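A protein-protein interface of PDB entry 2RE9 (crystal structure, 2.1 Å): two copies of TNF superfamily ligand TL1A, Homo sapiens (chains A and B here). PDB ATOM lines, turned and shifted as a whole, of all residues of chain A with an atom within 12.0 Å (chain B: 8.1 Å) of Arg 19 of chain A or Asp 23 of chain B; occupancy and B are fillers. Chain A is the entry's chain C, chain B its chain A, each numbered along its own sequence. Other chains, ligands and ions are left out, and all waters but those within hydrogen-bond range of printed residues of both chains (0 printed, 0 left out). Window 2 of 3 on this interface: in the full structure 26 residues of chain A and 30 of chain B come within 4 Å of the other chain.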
ATOM      1  N   LEU A  18      -8.104  -0.005 -31.061  1.00  0.00           N
ATOM      2  CA  LEU A  18      -8.515   0.980 -30.020  1.00  0.00           C
ATOM      3  C   LEU A  18      -8.848   0.284 -28.703  1.00  0.00           C
ATOM      4  O   LEU A  18      -9.319   0.922 -27.759  1.00  0.00           O
ATOM      5  CB  LEU A  18      -9.736   1.779 -30.494  1.00  0.00           C
ATOM      6  CG  LEU A  18      -9.594   2.705 -31.707  1.00  0.00           C
ATOM      7  CD1 LEU A  18      -9.246   1.902 -32.951  1.00  0.00           C
ATOM      8  CD2 LEU A  18     -10.898   3.458 -31.913  1.00  0.00           C
ATOM      9  N   ARG A  19      -8.603  -1.023 -28.642  1.00  0.00           N
ATOM     10  CA  ARG A  19      -8.884  -1.798 -27.436  1.00  0.00           C
ATOM     11  C   ARG A  19      -7.817  -2.859 -27.185  1.00  0.00           C
ATOM     12  O   ARG A  19      -7.003  -3.154 -28.061  1.00  0.00           O
ATOM     13  CB  ARG A  19     -10.259  -2.463 -27.551  1.00  0.00           C
ATOM     14  CG  ARG A  19     -11.392  -1.483 -27.813  1.00  0.00           C
ATOM     15  CD  ARG A  19     -12.736  -2.181 -27.926  1.00  0.00           C
ATOM     16  NE  ARG A  19     -13.794  -1.252 -28.315  1.00  0.00           N
ATOM     17  CZ  ARG A  19     -13.813  -0.581 -29.463  1.00  0.00           C
ATOM     18  NH1 ARG A  19     -14.813   0.244 -29.739  1.00  0.00           N
ATOM     19  NH2 ARG A  19     -12.832  -0.738 -30.338  1.00  0.00           N
ATOM     20  N   ALA A  20      -7.826  -3.431 -25.985  1.00  0.00           N
ATOM     21  CA  ALA A  20      -6.856  -4.455 -25.616  1.00  0.00           C
ATOM     22  C   ALA A  20      -7.526  -5.797 -25.335  1.00  0.00           C
ATOM     23  O   ALA A  20      -6.850  -6.791 -25.064  1.00  0.00           O
ATOM     24  CB  ALA A  20      -6.064  -4.003 -24.394  1.00  0.00           C
ATOM     25  N   ASP A  21      -8.853  -5.823 -25.399  1.00  0.00           N
ATOM     26  CA  ASP A  21      -9.600  -7.051 -25.156  1.00  0.00           C
ATOM     27  C   ASP A  21      -9.557  -7.947 -26.389  1.00  0.00           C
ATOM     28  O   ASP A  21     -10.217  -8.984 -26.441  1.00  0.00           O
ATOM     29  CB  ASP A  21     -11.054  -6.732 -24.793  1.00  0.00           C
ATOM     30  CG  ASP A  21     -11.779  -5.974 -25.887  1.00  0.00           C
ATOM     31  OD1 ASP A  21     -11.907  -6.514 -27.007  1.00  0.00           O
ATOM     32  OD2 ASP A  21     -12.224  -4.836 -25.626  1.00  0.00           O
ATOM     33  N   GLY A  22      -8.774  -7.534 -27.382  1.00  0.00           N
ATOM     34  CA  GLY A  22      -8.652  -8.315 -28.598  1.00  0.00           C
ATOM     35  C   GLY A  22      -7.643  -9.431 -28.426  1.00  0.00           C
ATOM     36  O   GLY A  22      -7.344 -10.165 -29.370  1.00  0.00           O
ATOM     37  N   ASP A  23      -7.114  -9.553 -27.212  1.00  0.00           N
ATOM     38  CA  ASP A  23      -6.130 -10.581 -26.889  1.00  0.00           C
ATOM     39  C   ASP A  23      -6.813 -11.817 -26.313  1.00  0.00           C
ATOM     40  O   ASP A  23      -6.156 -12.709 -25.778  1.00  0.00           O
ATOM     41  CB  ASP A  23      -5.120 -10.040 -25.875  1.00  0.00           C
ATOM     42  CG  ASP A  23      -5.783  -9.533 -24.606  1.00  0.00           C
ATOM     43  OD1 ASP A  23      -5.058  -9.176 -23.654  1.00  0.00           O
ATOM     44  OD2 ASP A  23      -7.030  -9.486 -24.561  1.00  0.00           O
ATOM     45  N   LYS A  24      -8.135 -11.863 -26.424  1.00  0.00           N
ATOM     46  CA  LYS A  24      -8.906 -12.989 -25.909  1.00  0.00           C
ATOM     47  C   LYS A  24      -8.876 -14.186 -26.854  1.00  0.00           C
ATOM     48  O   LYS A  24      -8.981 -14.031 -28.070  1.00  0.00           O
ATOM     49  CB  LYS A  24     -10.355 -12.564 -25.675  1.00  0.00           C
ATOM     50  CG  LYS A  24     -10.509 -11.472 -24.641  1.00  0.00           C
ATOM     51  CD  LYS A  24     -11.963 -11.086 -24.457  1.00  0.00           C
ATOM     52  CE  LYS A  24     -12.108 -10.026 -23.379  1.00  0.00           C
ATOM     53  NZ  LYS A  24     -13.522  -9.604 -23.208  1.00  0.00           N
ATOM     54  N   ARG A  26      -9.718 -17.063 -29.263  1.00  0.00           N
ATOM     55  CA  ARG A  26     -10.802 -17.180 -30.230  1.00  0.00           C
ATOM     56  C   ARG A  26     -10.442 -18.160 -31.329  1.00  0.00           C
ATOM     57  O   ARG A  26      -9.265 -18.350 -31.639  1.00  0.00           O
ATOM     58  CB  ARG A  26     -11.087 -15.816 -30.864  1.00  0.00           C
ATOM     59  CG  ARG A  26     -11.566 -14.778 -29.883  1.00  0.00           C
ATOM     60  CD  ARG A  26     -11.560 -13.387 -30.473  1.00  0.00           C
ATOM     61  NE  ARG A  26     -12.030 -12.428 -29.483  1.00  0.00           N
ATOM     62  CZ  ARG A  26     -11.889 -11.113 -29.579  1.00  0.00           C
ATOM     63  NH1 ARG A  26     -12.357 -10.329 -28.616  1.00  0.00           N
ATOM     64  NH2 ARG A  26     -11.279 -10.582 -30.630  1.00  0.00           N
ATOM     65  N   LYS A  59      -6.470 -17.853 -32.636  1.00  0.00           N
ATOM     66  CA  LYS A  59      -5.588 -16.794 -32.178  1.00  0.00           C
ATOM     67  C   LYS A  59      -5.573 -16.690 -30.665  1.00  0.00           C
ATOM     68  O   LYS A  59      -6.368 -17.332 -29.971  1.00  0.00           O
ATOM     69  CB  LYS A  59      -6.033 -15.457 -32.774  1.00  0.00           C
ATOM     70  CG  LYS A  59      -7.413 -15.018 -32.315  1.00  0.00           C
ATOM     71  CD  LYS A  59      -8.024 -13.968 -33.234  1.00  0.00           C
ATOM     72  CE  LYS A  59      -7.329 -12.623 -33.140  1.00  0.00           C
ATOM     73  NZ  LYS A  59      -7.965 -11.639 -34.064  1.00  0.00           N
ATOM     74  N   ASN A  60      -4.650 -15.876 -30.171  1.00  0.00           N
ATOM     75  CA  ASN A  60      -4.495 -15.622 -28.751  1.00  0.00           C
ATOM     76  C   ASN A  60      -4.445 -16.861 -27.873  1.00  0.00           C
ATOM     77  O   ASN A  60      -5.133 -16.934 -26.860  1.00  0.00           O
ATOM     78  CB  ASN A  60      -5.611 -14.689 -28.291  1.00  0.00           C
ATOM     79  CG  ASN A  60      -5.591 -13.366 -29.030  1.00  0.00           C
ATOM     80  OD1 ASN A  60      -6.579 -12.635 -29.049  1.00  0.00           O
ATOM     81  ND2 ASN A  60      -4.455 -13.050 -29.641  1.00  0.00           N
ATOM     82  N   LEU A 181     -15.476 -14.732 -23.413  1.00  0.00           N
ATOM     83  CA  LEU A 181     -16.334 -13.588 -23.309  1.00  0.00           C
ATOM     84  C   LEU A 181     -15.690 -12.398 -22.650  1.00  0.00           C
ATOM     85  O   LEU A 181     -15.045 -12.530 -21.650  1.00  0.00           O
ATOM     86  CB  LEU A 181     -17.627 -13.935 -22.632  1.00  0.00           C
ATOM     87  CG  LEU A 181     -18.522 -14.725 -23.538  1.00  0.00           C
ATOM     88  CD1 LEU A 181     -19.641 -15.266 -22.789  1.00  0.00           C
ATOM     89  CD2 LEU A 181     -19.001 -13.865 -24.602  1.00  0.00           C
ATOM     90  OXT LEU A 181     -15.938 -11.238 -22.778  1.00  0.00           O
ATOM     91  N   ARG B  19     -19.821   0.316 -18.435  1.00  0.00           N
ATOM     92  CA  ARG B  19     -18.619  -0.444 -18.771  1.00  0.00           C
ATOM     93  C   ARG B  19     -17.718   0.365 -19.703  1.00  0.00           C
ATOM     94  O   ARG B  19     -18.200   1.124 -20.544  1.00  0.00           O
ATOM     95  CB  ARG B  19     -19.002  -1.764 -19.449  1.00  0.00           C
ATOM     96  CG  ARG B  19     -19.635  -2.801 -18.528  1.00  0.00           C
ATOM     97  CD  ARG B  19     -18.614  -3.390 -17.565  1.00  0.00           C
ATOM     98  NE  ARG B  19     -19.180  -4.458 -16.746  1.00  0.00           N
ATOM     99  CZ  ARG B  19     -20.151  -4.285 -15.855  1.00  0.00           C
ATOM    100  NH1 ARG B  19     -20.605  -5.315 -15.157  1.00  0.00           N
ATOM    101  NH2 ARG B  19     -20.664  -3.080 -15.658  1.00  0.00           N
ATOM    102  N   ALA B  20     -16.407   0.197 -19.551  1.00  0.00           N
ATOM    103  CA  ALA B  20     -15.444   0.913 -20.382  1.00  0.00           C
ATOM    104  C   ALA B  20     -15.456   0.383 -21.816  1.00  0.00           C
ATOM    105  O   ALA B  20     -15.346   1.151 -22.774  1.00  0.00           O
ATOM    106  CB  ALA B  20     -14.046   0.783 -19.788  1.00  0.00           C
ATOM    107  N   ASP B  21     -15.594  -0.933 -21.951  1.00  0.00           N
ATOM    108  CA  ASP B  21     -15.623  -1.582 -23.260  1.00  0.00           C
ATOM    109  C   ASP B  21     -17.051  -1.709 -23.786  1.00  0.00           C
ATOM    110  O   ASP B  21     -17.533  -2.816 -24.040  1.00  0.00           O
ATOM    111  CB  ASP B  21     -14.985  -2.973 -23.165  1.00  0.00           C
ATOM    112  CG  ASP B  21     -15.664  -3.859 -22.132  1.00  0.00           C
ATOM    113  OD1 ASP B  21     -15.271  -5.039 -22.005  1.00  0.00           O
ATOM    114  OD2 ASP B  21     -16.589  -3.377 -21.443  1.00  0.00           O
ATOM    115  N   GLY B  22     -17.722  -0.573 -23.955  1.00  0.00           N
ATOM    116  CA  GLY B  22     -19.089  -0.591 -24.446  1.00  0.00           C
ATOM    117  C   GLY B  22     -19.285   0.200 -25.724  1.00  0.00           C
ATOM    118  O   GLY B  22     -20.339   0.116 -26.357  1.00  0.00           O
ATOM    119  N   ASP B  23     -18.272   0.974 -26.105  1.00  0.00           N
ATOM    120  CA  ASP B  23     -18.334   1.783 -27.317  1.00  0.00           C
ATOM    121  C   ASP B  23     -18.066   0.942 -28.564  1.00  0.00           C
ATOM    122  O   ASP B  23     -17.562   1.448 -29.561  1.00  0.00           O
ATOM    123  CB  ASP B  23     -17.305   2.913 -27.239  1.00  0.00           C
ATOM    124  CG  ASP B  23     -15.919   2.411 -26.867  1.00  0.00           C
ATOM    125  OD1 ASP B  23     -15.442   1.450 -27.508  1.00  0.00           O
ATOM    126  OD2 ASP B  23     -15.304   2.976 -25.936  1.00  0.00           O
ATOM    127  N   LYS B  24     -18.409  -0.340 -28.502  1.00  0.00           N
ATOM    128  CA  LYS B  24     -18.192  -1.251 -29.619  1.00  0.00           C
ATOM    129  C   LYS B  24     -19.325  -1.253 -30.648  1.00  0.00           C
ATOM    130  O   LYS B  24     -20.502  -1.208 -30.291  1.00  0.00           O
ATOM    131  CB  LYS B  24     -17.978  -2.668 -29.085  1.00  0.00           C
ATOM    132  CG  LYS B  24     -16.788  -2.773 -28.150  1.00  0.00           C
ATOM    133  CD  LYS B  24     -16.539  -4.199 -27.716  1.00  0.00           C
ATOM    134  CE  LYS B  24     -15.352  -4.271 -26.770  1.00  0.00           C
ATOM    135  NZ  LYS B  24     -15.022  -5.674 -26.394  1.00  0.00           N
ATOM    136  N   PRO B  25     -18.975  -1.306 -31.947  1.00  0.00           N
ATOM    137  CA  PRO B  25     -19.954  -1.316 -33.042  1.00  0.00           C
ATOM    138  C   PRO B  25     -20.931  -2.477 -32.883  1.00  0.00           C
ATOM    139  O   PRO B  25     -20.515  -3.627 -32.708  1.00  0.00           O
ATOM    140  CB  PRO B  25     -19.084  -1.479 -34.288  1.00  0.00           C
ATOM    141  CG  PRO B  25     -17.777  -0.858 -33.873  1.00  0.00           C
ATOM    142  CD  PRO B  25     -17.603  -1.383 -32.475  1.00  0.00           C
ATOM    143  N   ARG B  26     -22.223  -2.173 -32.952  1.00  0.00           N
ATOM    144  CA  ARG B  26     -23.263  -3.182 -32.805  1.00  0.00           C
ATOM    145  C   ARG B  26     -24.492  -2.807 -33.605  1.00  0.00           C
ATOM    146  O   ARG B  26     -24.765  -1.632 -33.828  1.00  0.00           O
ATOM    147  CB  ARG B  26     -23.680  -3.309 -31.332  1.00  0.00           C
ATOM    148  CG  ARG B  26     -22.572  -3.750 -30.418  1.00  0.00           C
ATOM    149  CD  ARG B  26     -22.940  -3.567 -28.969  1.00  0.00           C
ATOM    150  NE  ARG B  26     -21.839  -4.006 -28.122  1.00  0.00           N
ATOM    151  CZ  ARG B  26     -21.608  -3.553 -26.897  1.00  0.00           C
ATOM    152  NH1 ARG B  26     -20.574  -4.018 -26.211  1.00  0.00           N
ATOM    153  NH2 ARG B  26     -22.406  -2.635 -26.363  1.00  0.00           N
ATOM    154  N   LYS B  59     -25.525   1.280 -33.704  1.00  0.00           N
ATOM    155  CA  LYS B  59     -24.913   2.207 -32.772  1.00  0.00           C
ATOM    156  C   LYS B  59     -23.410   2.070 -32.811  1.00  0.00           C
ATOM    157  O   LYS B  59     -22.881   1.102 -33.344  1.00  0.00           O
ATOM    158  CB  LYS B  59     -25.399   1.913 -31.353  1.00  0.00           C
ATOM    159  CG  LYS B  59     -24.921   0.560 -30.829  1.00  0.00           C
ATOM    160  CD  LYS B  59     -25.625   0.150 -29.535  1.00  0.00           C
ATOM    161  CE  LYS B  59     -25.249   1.031 -28.362  1.00  0.00           C
ATOM    162  NZ  LYS B  59     -25.965   0.630 -27.116  1.00  0.00           N
ATOM    163  N   ASN B  60     -22.733   3.047 -32.225  1.00  0.00           N
ATOM    164  CA  ASN B  60     -21.283   3.066 -32.153  1.00  0.00           C
ATOM    165  C   ASN B  60     -20.578   2.915 -33.499  1.00  0.00           C
ATOM    166  O   ASN B  60     -19.616   2.153 -33.622  1.00  0.00           O
ATOM    167  CB  ASN B  60     -20.793   1.991 -31.184  1.00  0.00           C
ATOM    168  CG  ASN B  60     -21.399   2.139 -29.800  1.00  0.00           C
ATOM    169  OD1 ASN B  60     -21.813   3.227 -29.406  1.00  0.00           O
ATOM    170  ND2 ASN B  60     -21.435   1.045 -29.045  1.00  0.00           N
ATOM    171  N   ARG B  61     -21.074   3.638 -34.499  1.00  0.00           N
ATOM    172  CA  ARG B  61     -20.482   3.648 -35.838  1.00  0.00           C
ATOM    173  C   ARG B  61     -20.892   2.528 -36.784  1.00  0.00           C
ATOM    174  O   ARG B  61     -20.567   2.580 -37.974  1.00  0.00           O
ATOM    175  CB  ARG B  61     -18.957   3.679 -35.732  1.00  0.00           C
ATOM    176  CG  ARG B  61     -18.390   4.957 -35.119  1.00  0.00           C
ATOM    177  CD  ARG B  61     -16.971   4.716 -34.601  1.00  0.00           C
ATOM    178  NE  ARG B  61     -16.989   4.012 -33.318  1.00  0.00           N
ATOM    179  CZ  ARG B  61     -16.221   2.969 -33.009  1.00  0.00           C
ATOM    180  NH1 ARG B  61     -15.356   2.481 -33.891  1.00  0.00           N
ATOM    181  NH2 ARG B  61     -16.318   2.417 -31.807  1.00  0.00           N
ATOM    182  N   MET B  62     -21.580   1.507 -36.280  1.00  0.00           N
ATOM    183  CA  MET B  62     -22.008   0.437 -37.168  1.00  0.00           C
ATOM    184  C   MET B  62     -22.911   1.175 -38.141  1.00  0.00           C
ATOM    185  O   MET B  62     -23.723   1.996 -37.733  1.00  0.00           O
ATOM    186  CB  MET B  62     -22.785  -0.638 -36.406  1.00  0.00           C
ATOM    187  CG  MET B  62     -23.117  -1.860 -37.252  1.00  0.00           C
ATOM    188  SD  MET B  62     -21.654  -2.775 -37.812  1.00  0.00           S
ATOM    189  CE  MET B  62     -21.456  -3.970 -36.492  1.00  0.00           C
ATOM    190  N   PRO B  72     -17.214  -0.521 -39.343  1.00  0.00           N
ATOM    191  CA  PRO B  72     -16.444   0.698 -39.079  1.00  0.00           C
ATOM    192  C   PRO B  72     -15.091   0.485 -38.420  1.00  0.00           C
ATOM    193  O   PRO B  72     -14.257   1.384 -38.417  1.00  0.00           O
ATOM    194  CB  PRO B  72     -17.374   1.477 -38.171  1.00  0.00           C
ATOM    195  CG  PRO B  72     -17.871   0.369 -37.271  1.00  0.00           C
ATOM    196  CD  PRO B  72     -18.185  -0.760 -38.259  1.00  0.00           C
ATOM    197  N   GLU B  73     -14.874  -0.699 -37.864  1.00  0.00           N
ATOM    198  CA  GLU B  73     -13.627  -0.981 -37.167  1.00  0.00           C
ATOM    199  C   GLU B  73     -13.161  -2.413 -37.390  1.00  0.00           C
ATOM    200  O   GLU B  73     -13.946  -3.352 -37.280  1.00  0.00           O
ATOM    201  CB  GLU B  73     -13.827  -0.737 -35.668  1.00  0.00           C
ATOM    202  CG  GLU B  73     -12.569  -0.833 -34.837  1.00  0.00           C
ATOM    203  CD  GLU B  73     -12.858  -0.844 -33.346  1.00  0.00           C
ATOM    204  OE1 GLU B  73     -13.720  -0.057 -32.900  1.00  0.00           O
ATOM    205  OE2 GLU B  73     -12.212  -1.633 -32.622  1.00  0.00           O
ATOM    206  N   SER B  74     -11.881  -2.581 -37.693  1.00  0.00           N
ATOM    207  CA  SER B  74     -11.331  -3.906 -37.923  1.00  0.00           C
ATOM    208  C   SER B  74     -11.276  -4.715 -36.632  1.00  0.00           C
ATOM    209  O   SER B  74     -10.911  -4.196 -35.579  1.00  0.00           O
ATOM    210  CB  SER B  74      -9.927  -3.801 -38.526  1.00  0.00           C
ATOM    211  OG  SER B  74      -9.983  -3.240 -39.825  1.00  0.00           O
ATOM    212  N   TYR B  77     -15.840 -10.109 -35.247  1.00  0.00           N
ATOM    213  CA  TYR B  77     -17.254  -9.870 -35.005  1.00  0.00           C
ATOM    214  C   TYR B  77     -18.042 -11.164 -34.965  1.00  0.00           C
ATOM    215  O   TYR B  77     -17.656 -12.159 -35.574  1.00  0.00           O
ATOM    216  CB  TYR B  77     -17.870  -9.007 -36.112  1.00  0.00           C
ATOM    217  CG  TYR B  77     -17.421  -7.564 -36.156  1.00  0.00           C
ATOM    218  CD1 TYR B  77     -16.110  -7.224 -36.497  1.00  0.00           C
ATOM    219  CD2 TYR B  77     -18.319  -6.535 -35.878  1.00  0.00           C
ATOM    220  CE1 TYR B  77     -15.705  -5.881 -36.563  1.00  0.00           C
ATOM    221  CE2 TYR B  77     -17.928  -5.201 -35.937  1.00  0.00           C
ATOM    222  CZ  TYR B  77     -16.620  -4.882 -36.280  1.00  0.00           C
ATOM    223  OH  TYR B  77     -16.242  -3.560 -36.325  1.00  0.00           O
ATOM    224  N   LEU B 180     -19.008  -6.335 -32.476  1.00  0.00           N
ATOM    225  CA  LEU B 180     -17.568  -6.493 -32.300  1.00  0.00           C
ATOM    226  C   LEU B 180     -17.324  -7.181 -30.957  1.00  0.00           C
ATOM    227  O   LEU B 180     -17.875  -6.768 -29.938  1.00  0.00           O
ATOM    228  CB  LEU B 180     -16.884  -5.121 -32.301  1.00  0.00           C
ATOM    229  CG  LEU B 180     -15.393  -5.102 -31.946  1.00  0.00           C
ATOM    230  CD1 LEU B 180     -14.596  -5.759 -33.068  1.00  0.00           C
ATOM    231  CD2 LEU B 180     -14.926  -3.666 -31.732  1.00  0.00           C
ATOM    232  N   LEU B 181     -16.503  -8.201 -30.953  1.00  0.00           N
ATOM    233  CA  LEU B 181     -16.246  -8.947 -29.766  1.00  0.00           C
ATOM    234  C   LEU B 181     -15.407  -8.176 -28.767  1.00  0.00           C
ATOM    235  O   LEU B 181     -14.524  -7.447 -29.145  1.00  0.00           O
ATOM    236  CB  LEU B 181     -15.600 -10.266 -30.110  1.00  0.00           C
ATOM    237  CG  LEU B 181     -16.484 -11.491 -30.117  1.00  0.00           C
ATOM    238  CD1 LEU B 181     -17.942 -11.199 -29.987  1.00  0.00           C
ATOM    239  CD2 LEU B 181     -16.180 -12.371 -31.236  1.00  0.00           C
ATOM    240  OXT LEU B 181     -15.407  -8.220 -27.579  1.00  0.00           O
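The chain-end carboxylate (O) of Leu 181 of chain B is in salt-bridge range of the guanidinium group (NH1) of Arg 26 of chain A. The side-chain carboxylate (OD1) of Asp 23 of chain B is in salt-bridge range of the guanidinium group (NH1) of Arg 19 of chain A. The guanidinium group (NH1) of Arg 19 of chain A lies close to the guanidinium group (NH2) of Arg 61 of chain B (3.4 Å). The guanidinium group (NH2) of Arg 19 of chain A lies within salt-bridge range of the side-chain carboxylate (OE2) of Glu 73 of chain B, 2.5 Å away. The side-chain amino group (NZ) of Lys 24 of chain B lies within salt-bridge range of the side-chain carboxylate (OD2) of Asp 21 of chain A, 3.0 Å away.
The backbone carbonyl oxygen of Arg 26 of chain A lies within hydrogen-bond range of the backbone NH of Lys 59 of chain A. The side-chain carboxylate (OE1) of Glu 73 of chain B is in salt-bridge range of the guanidinium group (NH1) of Arg 61 of chain B, at 3.2 Å. The guanidinium group (NH2) of Arg 61 of chain B sits at hydrogen-bond distance from the backbone carbonyl oxygen (O) of Asp 23 of chain B (2.7 Å). The side-chain amino group (NZ) of Lys 24 of chain B lies within salt-bridge range of the chain-end carboxylate (OXT) of Leu 181 of chain B (2.8 Å). O of Pro 25 of chain B lies within hydrogen-bond range of N of Leu 180 of chain B (3.1 Å). OH of Tyr 77 of chain B sits at hydrogen-bond distance from O of Glu 73 of chain B, 2.5 Å away.
Among the printed residues, merely in contact across the chains: Arg 19 of chain A with Lys 24 of chain B (3.4 Å), Arg 19 of chain A with Leu 180 of chain B (3.9 Å) and Asp 21 of chain A with Leu 181 of chain B (3.5 Å).
Asp 23 of chain B touches just one residue of chain A: Arg 19 (2.6 Å). No residue of chain A comes within 4 Å of Ala 20 of chain B. No residue of chain A comes within 4 Å of Asp 21 of chain B. Gly 22 of chain B touches none of the printed residues of chain A. Lys 24 of chain B touches two residues of chain A. No residue of chain A comes within 4 Å of Pro 25 of chain B. Glu 73 of chain B touches just one residue of chain A: Arg 19 (2.5 Å). Of the printed residues of chain A, Arg 61 of chain B touches Arg 19 (3.4 Å). Of the printed residues of chain B, Arg 26 of chain A touches Leu 181 (3.6 Å). Of the printed residues of chain A, Leu 180 of chain B touches Arg 19. Of the printed residues of chain B, Asp 21 of chain A touches Lys 24 and Leu 181. Lys 59 of chain A touches none of the printed residues of chain B. Arg 19 of chain B touches none of the printed residues of chain A. The nearest residue of chain B that does not touch Arg 19 of chain A is Pro 25 of chain B (4.2 Å). The nearest printed residue of chain B that does not touch Asp 21 of chain A is Asp 21 of chain B (4.1 Å).
Hydrophobic or aromatic side chains of chain B that line the printed part of chain A: Leu 180 and Leu 181. Along chain A the printed residues that touch a printed residue of chain B span positions 19 to 26. Among the printed residues, 8 pairs touch across the chains. Among the printed residues, Asp or Glu carboxylates within 4 Å of a Lys or Arg side-chain nitrogen of the other chain: Arg 19 of chain A with Asp 23 of chain B, Arg 19 of chain A with Glu 73 of chain B and Asp 21 of chain A with Lys 24 of chain B.
Arg 19 of chain A touches Asp 23 of chain B, but with the chains exchanged Asp 23 of chain A does not touch Arg 19 of chain B (14.8 Å). Arg 19 of chain A touches Lys 24 of chain B, but with the chains exchanged Lys 24 of chain A does not touch Arg 19 of chain B (9.8 Å). Asp 21 of chain A touches Leu 181 of chain B, but with the chains exchanged Leu 181 of chain A does not touch Asp 21 of chain B (6.3 Å). Arg 26 of chain A touches Leu 181 of chain B, but with the chains exchanged Leu 181 of chain A does not touch Arg 26 of chain B (9.2 Å). Positions printed for both chains: 19, 20, 21, 22, 23, 24, 26, 59, 60 and 181.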
